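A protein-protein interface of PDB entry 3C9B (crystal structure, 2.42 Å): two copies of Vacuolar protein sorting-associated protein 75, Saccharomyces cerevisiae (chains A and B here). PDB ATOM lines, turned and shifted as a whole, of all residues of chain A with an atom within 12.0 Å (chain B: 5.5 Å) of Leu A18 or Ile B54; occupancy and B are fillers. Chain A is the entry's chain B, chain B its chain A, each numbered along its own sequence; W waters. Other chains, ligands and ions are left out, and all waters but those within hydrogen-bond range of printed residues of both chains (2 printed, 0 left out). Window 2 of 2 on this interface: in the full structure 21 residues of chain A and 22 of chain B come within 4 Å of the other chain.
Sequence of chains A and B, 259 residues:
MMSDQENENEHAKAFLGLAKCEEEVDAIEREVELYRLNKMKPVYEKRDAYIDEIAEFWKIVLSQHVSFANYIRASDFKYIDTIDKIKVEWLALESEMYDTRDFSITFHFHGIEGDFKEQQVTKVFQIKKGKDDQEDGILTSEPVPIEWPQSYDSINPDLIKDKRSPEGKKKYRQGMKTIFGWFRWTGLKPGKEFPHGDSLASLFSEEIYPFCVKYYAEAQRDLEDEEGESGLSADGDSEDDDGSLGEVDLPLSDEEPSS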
ATOM      1  N   GLY A  17     -16.015  -9.380  20.713  1.00  0.00           N
ATOM      2  CA  GLY A  17     -17.198 -10.065  20.116  1.00  0.00           C
ATOM      3  C   GLY A  17     -16.903 -11.505  19.742  1.00  0.00           C
ATOM      4  O   GLY A  17     -17.175 -12.425  20.519  1.00  0.00           O
ATOM      5  N   LEU A  18     -16.342 -11.697  18.548  1.00  0.00           N
ATOM      6  CA  LEU A  18     -15.974 -13.025  18.055  1.00  0.00           C
ATOM      7  C   LEU A  18     -14.900 -13.695  18.922  1.00  0.00           C
ATOM      8  O   LEU A  18     -14.931 -14.913  19.128  1.00  0.00           O
ATOM      9  CB  LEU A  18     -15.504 -12.951  16.599  1.00  0.00           C
ATOM     10  CG  LEU A  18     -16.513 -12.571  15.505  1.00  0.00           C
ATOM     11  CD1 LEU A  18     -15.798 -12.384  14.185  1.00  0.00           C
ATOM     12  CD2 LEU A  18     -17.616 -13.603  15.360  1.00  0.00           C
ATOM     13  N   ALA A  19     -13.963 -12.892  19.431  1.00  0.00           N
ATOM     14  CA  ALA A  19     -12.921 -13.373  20.341  1.00  0.00           C
ATOM     15  C   ALA A  19     -13.484 -13.918  21.657  1.00  0.00           C
ATOM     16  O   ALA A  19     -12.981 -14.907  22.184  1.00  0.00           O
ATOM     17  CB  ALA A  19     -11.897 -12.279  20.607  1.00  0.00           C
ATOM     18  N   LYS A  20     -14.528 -13.273  22.174  1.00  0.00           N
ATOM     19  CA  LYS A  20     -15.162 -13.694  23.435  1.00  0.00           C
ATOM     20  C   LYS A  20     -15.958 -14.980  23.242  1.00  0.00           C
ATOM     21  O   LYS A  20     -16.015 -15.826  24.140  1.00  0.00           O
ATOM     22  CB  LYS A  20     -16.079 -12.595  23.998  1.00  0.00           C
ATOM     23  CG  LYS A  20     -15.743 -11.163  23.541  1.00  0.00           C
ATOM     24  CD  LYS A  20     -14.328 -10.742  23.955  1.00  0.00           C
ATOM     25  CE  LYS A  20     -13.670  -9.895  22.864  1.00  0.00           C
ATOM     26  NZ  LYS A  20     -12.190  -9.775  23.055  1.00  0.00           N
ATOM     27  N   CYS A  21     -16.570 -15.120  22.066  1.00  0.00           N
ATOM     28  CA  CYS A  21     -17.251 -16.353  21.685  1.00  0.00           C
ATOM     29  C   CYS A  21     -16.283 -17.515  21.597  1.00  0.00           C
ATOM     30  O   CYS A  21     -16.618 -18.617  21.997  1.00  0.00           O
ATOM     31  CB  CYS A  21     -17.981 -16.189  20.350  1.00  0.00           C
ATOM     32  SG  CYS A  21     -19.433 -15.136  20.416  1.00  0.00           S
ATOM     33  N   GLU A  22     -15.078 -17.257  21.080  1.00  0.00           N
ATOM     34  CA  GLU A  22     -14.059 -18.305  20.913  1.00  0.00           C
ATOM     35  C   GLU A  22     -13.559 -18.848  22.246  1.00  0.00           C
ATOM     36  O   GLU A  22     -13.271 -20.041  22.358  1.00  0.00           O
ATOM     37  CB  GLU A  22     -12.887 -17.822  20.051  1.00  0.00           C
ATOM     38  CG  GLU A  22     -13.243 -17.561  18.566  1.00  0.00           C
ATOM     39  CD  GLU A  22     -13.670 -18.826  17.797  1.00  0.00           C
ATOM     40  OE1 GLU A  22     -12.865 -19.786  17.713  1.00  0.00           O
ATOM     41  OE2 GLU A  22     -14.803 -18.846  17.258  1.00  0.00           O
ATOM     42  N   GLU A  23     -13.470 -17.970  23.248  1.00  0.00           N
ATOM     43  CA  GLU A  23     -13.105 -18.352  24.623  1.00  0.00           C
ATOM     44  C   GLU A  23     -14.207 -19.180  25.284  1.00  0.00           C
ATOM     45  O   GLU A  23     -13.924 -20.154  25.978  1.00  0.00           O
ATOM     46  CB  GLU A  23     -12.799 -17.107  25.477  1.00  0.00           C
ATOM     47  CG  GLU A  23     -11.455 -16.438  25.174  1.00  0.00           C
ATOM     48  CD  GLU A  23     -11.418 -14.941  25.551  1.00  0.00           C
ATOM     49  OE1 GLU A  23     -12.267 -14.489  26.364  1.00  0.00           O
ATOM     50  OE2 GLU A  23     -10.533 -14.214  25.030  1.00  0.00           O
ATOM     51  N   GLU A  24     -15.462 -18.776  25.062  1.00  0.00           N
ATOM     52  CA  GLU A  24     -16.640 -19.547  25.495  1.00  0.00           C
ATOM     53  C   GLU A  24     -16.626 -20.977  24.952  1.00  0.00           C
ATOM     54  O   GLU A  24     -16.891 -21.926  25.686  1.00  0.00           O
ATOM     55  CB  GLU A  24     -17.935 -18.843  25.074  1.00  0.00           C
ATOM     56  CG  GLU A  24     -18.818 -18.361  26.220  1.00  0.00           C
ATOM     57  CD  GLU A  24     -19.649 -17.127  25.841  1.00  0.00           C
ATOM     58  OE1 GLU A  24     -20.855 -17.287  25.531  1.00  0.00           O
ATOM     59  OE2 GLU A  24     -19.093 -15.996  25.843  1.00  0.00           O
ATOM     60  N   VAL A  25     -16.308 -21.119  23.666  1.00  0.00           N
ATOM     61  CA  VAL A  25     -16.231 -22.424  23.032  1.00  0.00           C
ATOM     62  C   VAL A  25     -15.199 -23.335  23.697  1.00  0.00           C
ATOM     63  O   VAL A  25     -15.475 -24.509  23.932  1.00  0.00           O
ATOM     64  CB  VAL A  25     -15.961 -22.314  21.511  1.00  0.00           C
ATOM     65  CG1 VAL A  25     -15.626 -23.682  20.922  1.00  0.00           C
ATOM     66  CG2 VAL A  25     -17.159 -21.710  20.802  1.00  0.00           C
ATOM     67  N   ASP A  26     -14.020 -22.789  24.002  1.00  0.00           N
ATOM     68  CA  ASP A  26     -12.979 -23.545  24.725  1.00  0.00           C
ATOM     69  C   ASP A  26     -13.409 -23.890  26.139  1.00  0.00           C
ATOM     70  O   ASP A  26     -13.167 -25.002  26.602  1.00  0.00           O
ATOM     71  CB  ASP A  26     -11.642 -22.798  24.742  1.00  0.00           C
ATOM     72  CG  ASP A  26     -10.969 -22.756  23.363  1.00  0.00           C
ATOM     73  OD1 ASP A  26     -11.543 -23.299  22.376  1.00  0.00           O
ATOM     74  OD2 ASP A  26      -9.864 -22.166  23.265  1.00  0.00           O
ATOM     75  N   ALA A  27     -14.057 -22.949  26.817  1.00  0.00           N
ATOM     76  CA  ALA A  27     -14.642 -23.232  28.121  1.00  0.00           C
ATOM     77  C   ALA A  27     -15.660 -24.386  28.040  1.00  0.00           C
ATOM     78  O   ALA A  27     -15.599 -25.341  28.827  1.00  0.00           O
ATOM     79  CB  ALA A  27     -15.271 -21.987  28.710  1.00  0.00           C
ATOM     80  N   ILE A  28     -16.568 -24.300  27.068  1.00  0.00           N
ATOM     81  CA  ILE A  28     -17.595 -25.322  26.858  1.00  0.00           C
ATOM     82  C   ILE A  28     -17.007 -26.705  26.520  1.00  0.00           C
ATOM     83  O   ILE A  28     -17.480 -27.718  27.033  1.00  0.00           O
ATOM     84  CB  ILE A  28     -18.644 -24.872  25.801  1.00  0.00           C
ATOM     85  CG1 ILE A  28     -19.556 -23.790  26.392  1.00  0.00           C
ATOM     86  CG2 ILE A  28     -19.489 -26.057  25.294  1.00  0.00           C
ATOM     87  CD1 ILE A  28     -20.217 -22.927  25.359  1.00  0.00           C
ATOM     88  N   ARG B  47     -22.341 -15.804  18.139  1.00  0.00           N
ATOM     89  CA  ARG B  47     -21.233 -15.689  17.193  1.00  0.00           C
ATOM     90  C   ARG B  47     -21.716 -15.255  15.814  1.00  0.00           C
ATOM     91  O   ARG B  47     -21.149 -14.344  15.223  1.00  0.00           O
ATOM     92  CB  ARG B  47     -20.439 -16.995  17.098  1.00  0.00           C
ATOM     93  CG  ARG B  47     -19.168 -16.915  16.248  1.00  0.00           C
ATOM     94  CD  ARG B  47     -18.746 -18.296  15.750  1.00  0.00           C
ATOM     95  NE  ARG B  47     -19.642 -18.810  14.701  1.00  0.00           N
ATOM     96  CZ  ARG B  47     -19.526 -20.007  14.116  1.00  0.00           C
ATOM     97  NH1 ARG B  47     -18.563 -20.853  14.479  1.00  0.00           N
ATOM     98  NH2 ARG B  47     -20.379 -20.357  13.167  1.00  0.00           N
ATOM     99  N   TYR B  50     -22.527 -11.554  15.149  1.00  0.00           N
ATOM    100  CA  TYR B  50     -21.353 -10.733  14.881  1.00  0.00           C
ATOM    101  C   TYR B  50     -20.875 -10.957  13.456  1.00  0.00           C
ATOM    102  O   TYR B  50     -20.529 -10.009  12.760  1.00  0.00           O
ATOM    103  CB  TYR B  50     -20.215 -11.055  15.858  1.00  0.00           C
ATOM    104  CG  TYR B  50     -20.459 -10.630  17.286  1.00  0.00           C
ATOM    105  CD1 TYR B  50     -20.688  -9.281  17.618  1.00  0.00           C
ATOM    106  CD2 TYR B  50     -20.426 -11.563  18.318  1.00  0.00           C
ATOM    107  CE1 TYR B  50     -20.901  -8.885  18.950  1.00  0.00           C
ATOM    108  CE2 TYR B  50     -20.638 -11.182  19.653  1.00  0.00           C
ATOM    109  CZ  TYR B  50     -20.873  -9.843  19.961  1.00  0.00           C
ATOM    110  OH  TYR B  50     -21.078  -9.478  21.279  1.00  0.00           O
ATOM    111  N   ILE B  51     -20.857 -12.223  13.035  1.00  0.00           N
ATOM    112  CA  ILE B  51     -20.442 -12.607  11.681  1.00  0.00           C
ATOM    113  C   ILE B  51     -21.298 -11.905  10.625  1.00  0.00           C
ATOM    114  O   ILE B  51     -20.795 -11.506   9.568  1.00  0.00           O
ATOM    115  CB  ILE B  51     -20.509 -14.156  11.479  1.00  0.00           C
ATOM    116  CG1 ILE B  51     -19.418 -14.853  12.305  1.00  0.00           C
ATOM    117  CG2 ILE B  51     -20.400 -14.520   9.993  1.00  0.00           C
ATOM    118  CD1 ILE B  51     -19.480 -16.380  12.299  1.00  0.00           C
ATOM    119  N   ASP B  52     -22.585 -11.744  10.927  1.00  0.00           N
ATOM    120  CA  ASP B  52     -23.524 -11.101  10.011  1.00  0.00           C
ATOM    121  C   ASP B  52     -23.228  -9.618   9.789  1.00  0.00           C
ATOM    122  O   ASP B  52     -23.785  -9.005   8.887  1.00  0.00           O
ATOM    123  CB  ASP B  52     -24.965 -11.281  10.501  1.00  0.00           C
ATOM    124  CG  ASP B  52     -25.472 -12.722  10.350  1.00  0.00           C
ATOM    125  OD1 ASP B  52     -24.806 -13.554   9.674  1.00  0.00           O
ATOM    126  OD2 ASP B  52     -26.544 -13.020  10.926  1.00  0.00           O
ATOM    127  N   GLU B  53     -22.360  -9.056  10.628  1.00  0.00           N
ATOM    128  CA  GLU B  53     -21.957  -7.650  10.532  1.00  0.00           C
ATOM    129  C   GLU B  53     -20.708  -7.493   9.661  1.00  0.00           C
ATOM    130  O   GLU B  53     -20.362  -6.381   9.275  1.00  0.00           O
ATOM    131  CB  GLU B  53     -21.675  -7.062  11.923  1.00  0.00           C
ATOM    132  CG  GLU B  53     -22.887  -6.933  12.853  1.00  0.00           C
ATOM    133  CD  GLU B  53     -22.494  -6.523  14.300  1.00  0.00           C
ATOM    134  OE1 GLU B  53     -23.075  -7.082  15.265  1.00  0.00           O
ATOM    135  OE2 GLU B  53     -21.608  -5.645  14.470  1.00  0.00           O
ATOM    136  N   ILE B  54     -20.037  -8.607   9.362  1.00  0.00           N
ATOM    137  CA  ILE B  54     -18.760  -8.587   8.629  1.00  0.00           C
ATOM    138  C   ILE B  54     -18.964  -8.875   7.150  1.00  0.00           C
ATOM    139  O   ILE B  54     -19.457  -9.945   6.771  1.00  0.00           O
ATOM    140  CB  ILE B  54     -17.712  -9.558   9.240  1.00  0.00           C
ATOM    141  CG1 ILE B  54     -17.491  -9.241  10.728  1.00  0.00           C
ATOM    142  CG2 ILE B  54     -16.386  -9.498   8.461  1.00  0.00           C
ATOM    143  CD1 ILE B  54     -16.488 -10.130  11.404  1.00  0.00           C
ATOM    144  N   ALA B  55     -18.534  -7.918   6.326  1.00  0.00           N
ATOM    145  CA  ALA B  55     -18.967  -7.779   4.927  1.00  0.00           C
ATOM    146  C   ALA B  55     -18.846  -9.042   4.087  1.00  0.00           C
ATOM    147  O   ALA B  55     -19.851  -9.564   3.575  1.00  0.00           O
ATOM    148  CB  ALA B  55     -18.222  -6.613   4.252  1.00  0.00           C
ATOM    149  N   GLU B  56     -17.621  -9.525   3.935  1.00  0.00           N
ATOM    150  CA  GLU B  56     -17.360 -10.632   3.035  1.00  0.00           C
ATOM    151  C   GLU B  56     -16.797 -11.814   3.810  1.00  0.00           C
ATOM    152  O   GLU B  56     -15.947 -12.557   3.303  1.00  0.00           O
ATOM    153  CB  GLU B  56     -16.411 -10.183   1.919  1.00  0.00           C
ATOM    154  CG  GLU B  56     -17.021  -9.127   0.981  1.00  0.00           C
ATOM    155  CD  GLU B  56     -16.055  -8.645  -0.115  1.00  0.00           C
ATOM    156  OE1 GLU B  56     -14.896  -9.143  -0.187  1.00  0.00           O
ATOM    157  OE2 GLU B  56     -16.464  -7.756  -0.908  1.00  0.00           O
ATOM    158  N   PHE B  57     -17.298 -11.988   5.038  1.00  0.00           N
ATOM    159  CA  PHE B  57     -16.790 -12.995   5.977  1.00  0.00           C
ATOM    160  C   PHE B  57     -16.682 -14.362   5.327  1.00  0.00           C
ATOM    161  O   PHE B  57     -15.610 -14.969   5.325  1.00  0.00           O
ATOM    162  CB  PHE B  57     -17.674 -13.063   7.229  1.00  0.00           C
ATOM    163  CG  PHE B  57     -17.212 -14.075   8.253  1.00  0.00           C
ATOM    164  CD1 PHE B  57     -16.286 -13.719   9.237  1.00  0.00           C
ATOM    165  CD2 PHE B  57     -17.714 -15.384   8.245  1.00  0.00           C
ATOM    166  CE1 PHE B  57     -15.855 -14.657  10.197  1.00  0.00           C
ATOM    167  CE2 PHE B  57     -17.292 -16.321   9.196  1.00  0.00           C
ATOM    168  CZ  PHE B  57     -16.357 -15.955  10.174  1.00  0.00           C
ATOM    169  N   VAL B 213     -14.249 -18.535  12.213  1.00  0.00           N
ATOM    170  CA  VAL B 213     -13.595 -17.358  12.786  1.00  0.00           C
ATOM    171  C   VAL B 213     -12.062 -17.517  12.811  1.00  0.00           C
ATOM    172  O   VAL B 213     -11.332 -16.546  12.587  1.00  0.00           O
ATOM    173  CB  VAL B 213     -14.162 -17.008  14.207  1.00  0.00           C
ATOM    174  CG1 VAL B 213     -13.446 -15.795  14.807  1.00  0.00           C
ATOM    175  CG2 VAL B 213     -15.642 -16.737  14.140  1.00  0.00           C
ATOM    176  N   TYR B 216     -10.973 -16.875   9.218  1.00  0.00           N
ATOM    177  CA  TYR B 216     -11.018 -15.442   8.968  1.00  0.00           C
ATOM    178  C   TYR B 216      -9.820 -14.737   9.624  1.00  0.00           C
ATOM    179  O   TYR B 216      -9.210 -13.837   9.024  1.00  0.00           O
ATOM    180  CB  TYR B 216     -12.333 -14.844   9.478  1.00  0.00           C
ATOM    181  CG  TYR B 216     -12.515 -13.390   9.125  1.00  0.00           C
ATOM    182  CD1 TYR B 216     -12.975 -13.007   7.858  1.00  0.00           C
ATOM    183  CD2 TYR B 216     -12.221 -12.388  10.051  1.00  0.00           C
ATOM    184  CE1 TYR B 216     -13.133 -11.667   7.526  1.00  0.00           C
ATOM    185  CE2 TYR B 216     -12.376 -11.042   9.729  1.00  0.00           C
ATOM    186  CZ  TYR B 216     -12.829 -10.688   8.467  1.00  0.00           C
ATOM    187  OH  TYR B 216     -12.989  -9.354   8.154  1.00  0.00           O
HETATM  188  O   HOH W   1     -14.957 -20.359  14.630  1.00  0.00           O
HETATM  189  O   HOH W   2     -16.965 -20.776  16.921  1.00  0.00           O
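SG of Cys A21 sits close to N of Arg B47, 3.8 Å away.
No position is printed for both chains.
Among the printed residues, pairs that only touch across the chains: Gly A17 with Tyr B50 (3.6 Å), Leu A18 with Arg B47 (3.6 Å), Leu A18 with Tyr B50 (3.7 Å), Leu A18 with Ile B51 (3.8 Å), Leu A18 with Ile B54 (3.6 Å), Leu A18 with Val B213 (3.9 Å) and Glu A22 with Val B213 (3.6 Å).
Hydrophobic or aromatic side chains of chain A that line the printed part of chain B: Leu A18.
Of the 11 printed residues of chain B, 5 touch a printed residue of chain A.
Hydrophobic or aromatic side chains of chain B that line the printed part of chain A: Tyr B50, Ile B51, Ile B54 and Val B213.
Among the printed residues, 8 pairs touch across the chains.
Water W2 lies within hydrogen-bond range of the side-chain carboxylate (OE2) of Glu A22 (2.9 Å) and the guanidinium group (NH1) of Arg B47 (2.9 Å).
Water W1 bridges OE2 of Glu A22 (3.0 Å) and N of Val B213 (3.1 Å).
The backbone carbonyl oxygen (O) of Gly A17 lies within hydrogen-bond range of the side-chain sulfur (SG) of Cys A21.
Of the printed residues of chain B, Gly A17 touches Tyr B50 (3.6 Å).
Of chain B, only Arg B47, Tyr B50, Ile B51, Ile B54 and Val B213 come within 4 Å of Leu A18.
Ala A19 touches none of the printed residues of chain B.
Printed residues of chain B within 4 Å of Cys A21: Arg B47.
Val A25 touches none of the printed residues of chain B.
Of chain A, only Gly A17 and Leu A18 come within 4 Å of Tyr B50.
Of chain A, only Leu A18 comes within 4 Å of Ile B51.
No residue of chain A comes within 4 Å of Glu B53.
Ile B54 touches one residue of chain A.
Ala B55 touches none of the printed residues of chain A.
No residue of chain A comes within 4 Å of Phe B57.
Val B213 touches just these residues of chain A: Leu A18 (3.9 Å) and Glu A22 (3.6 Å).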
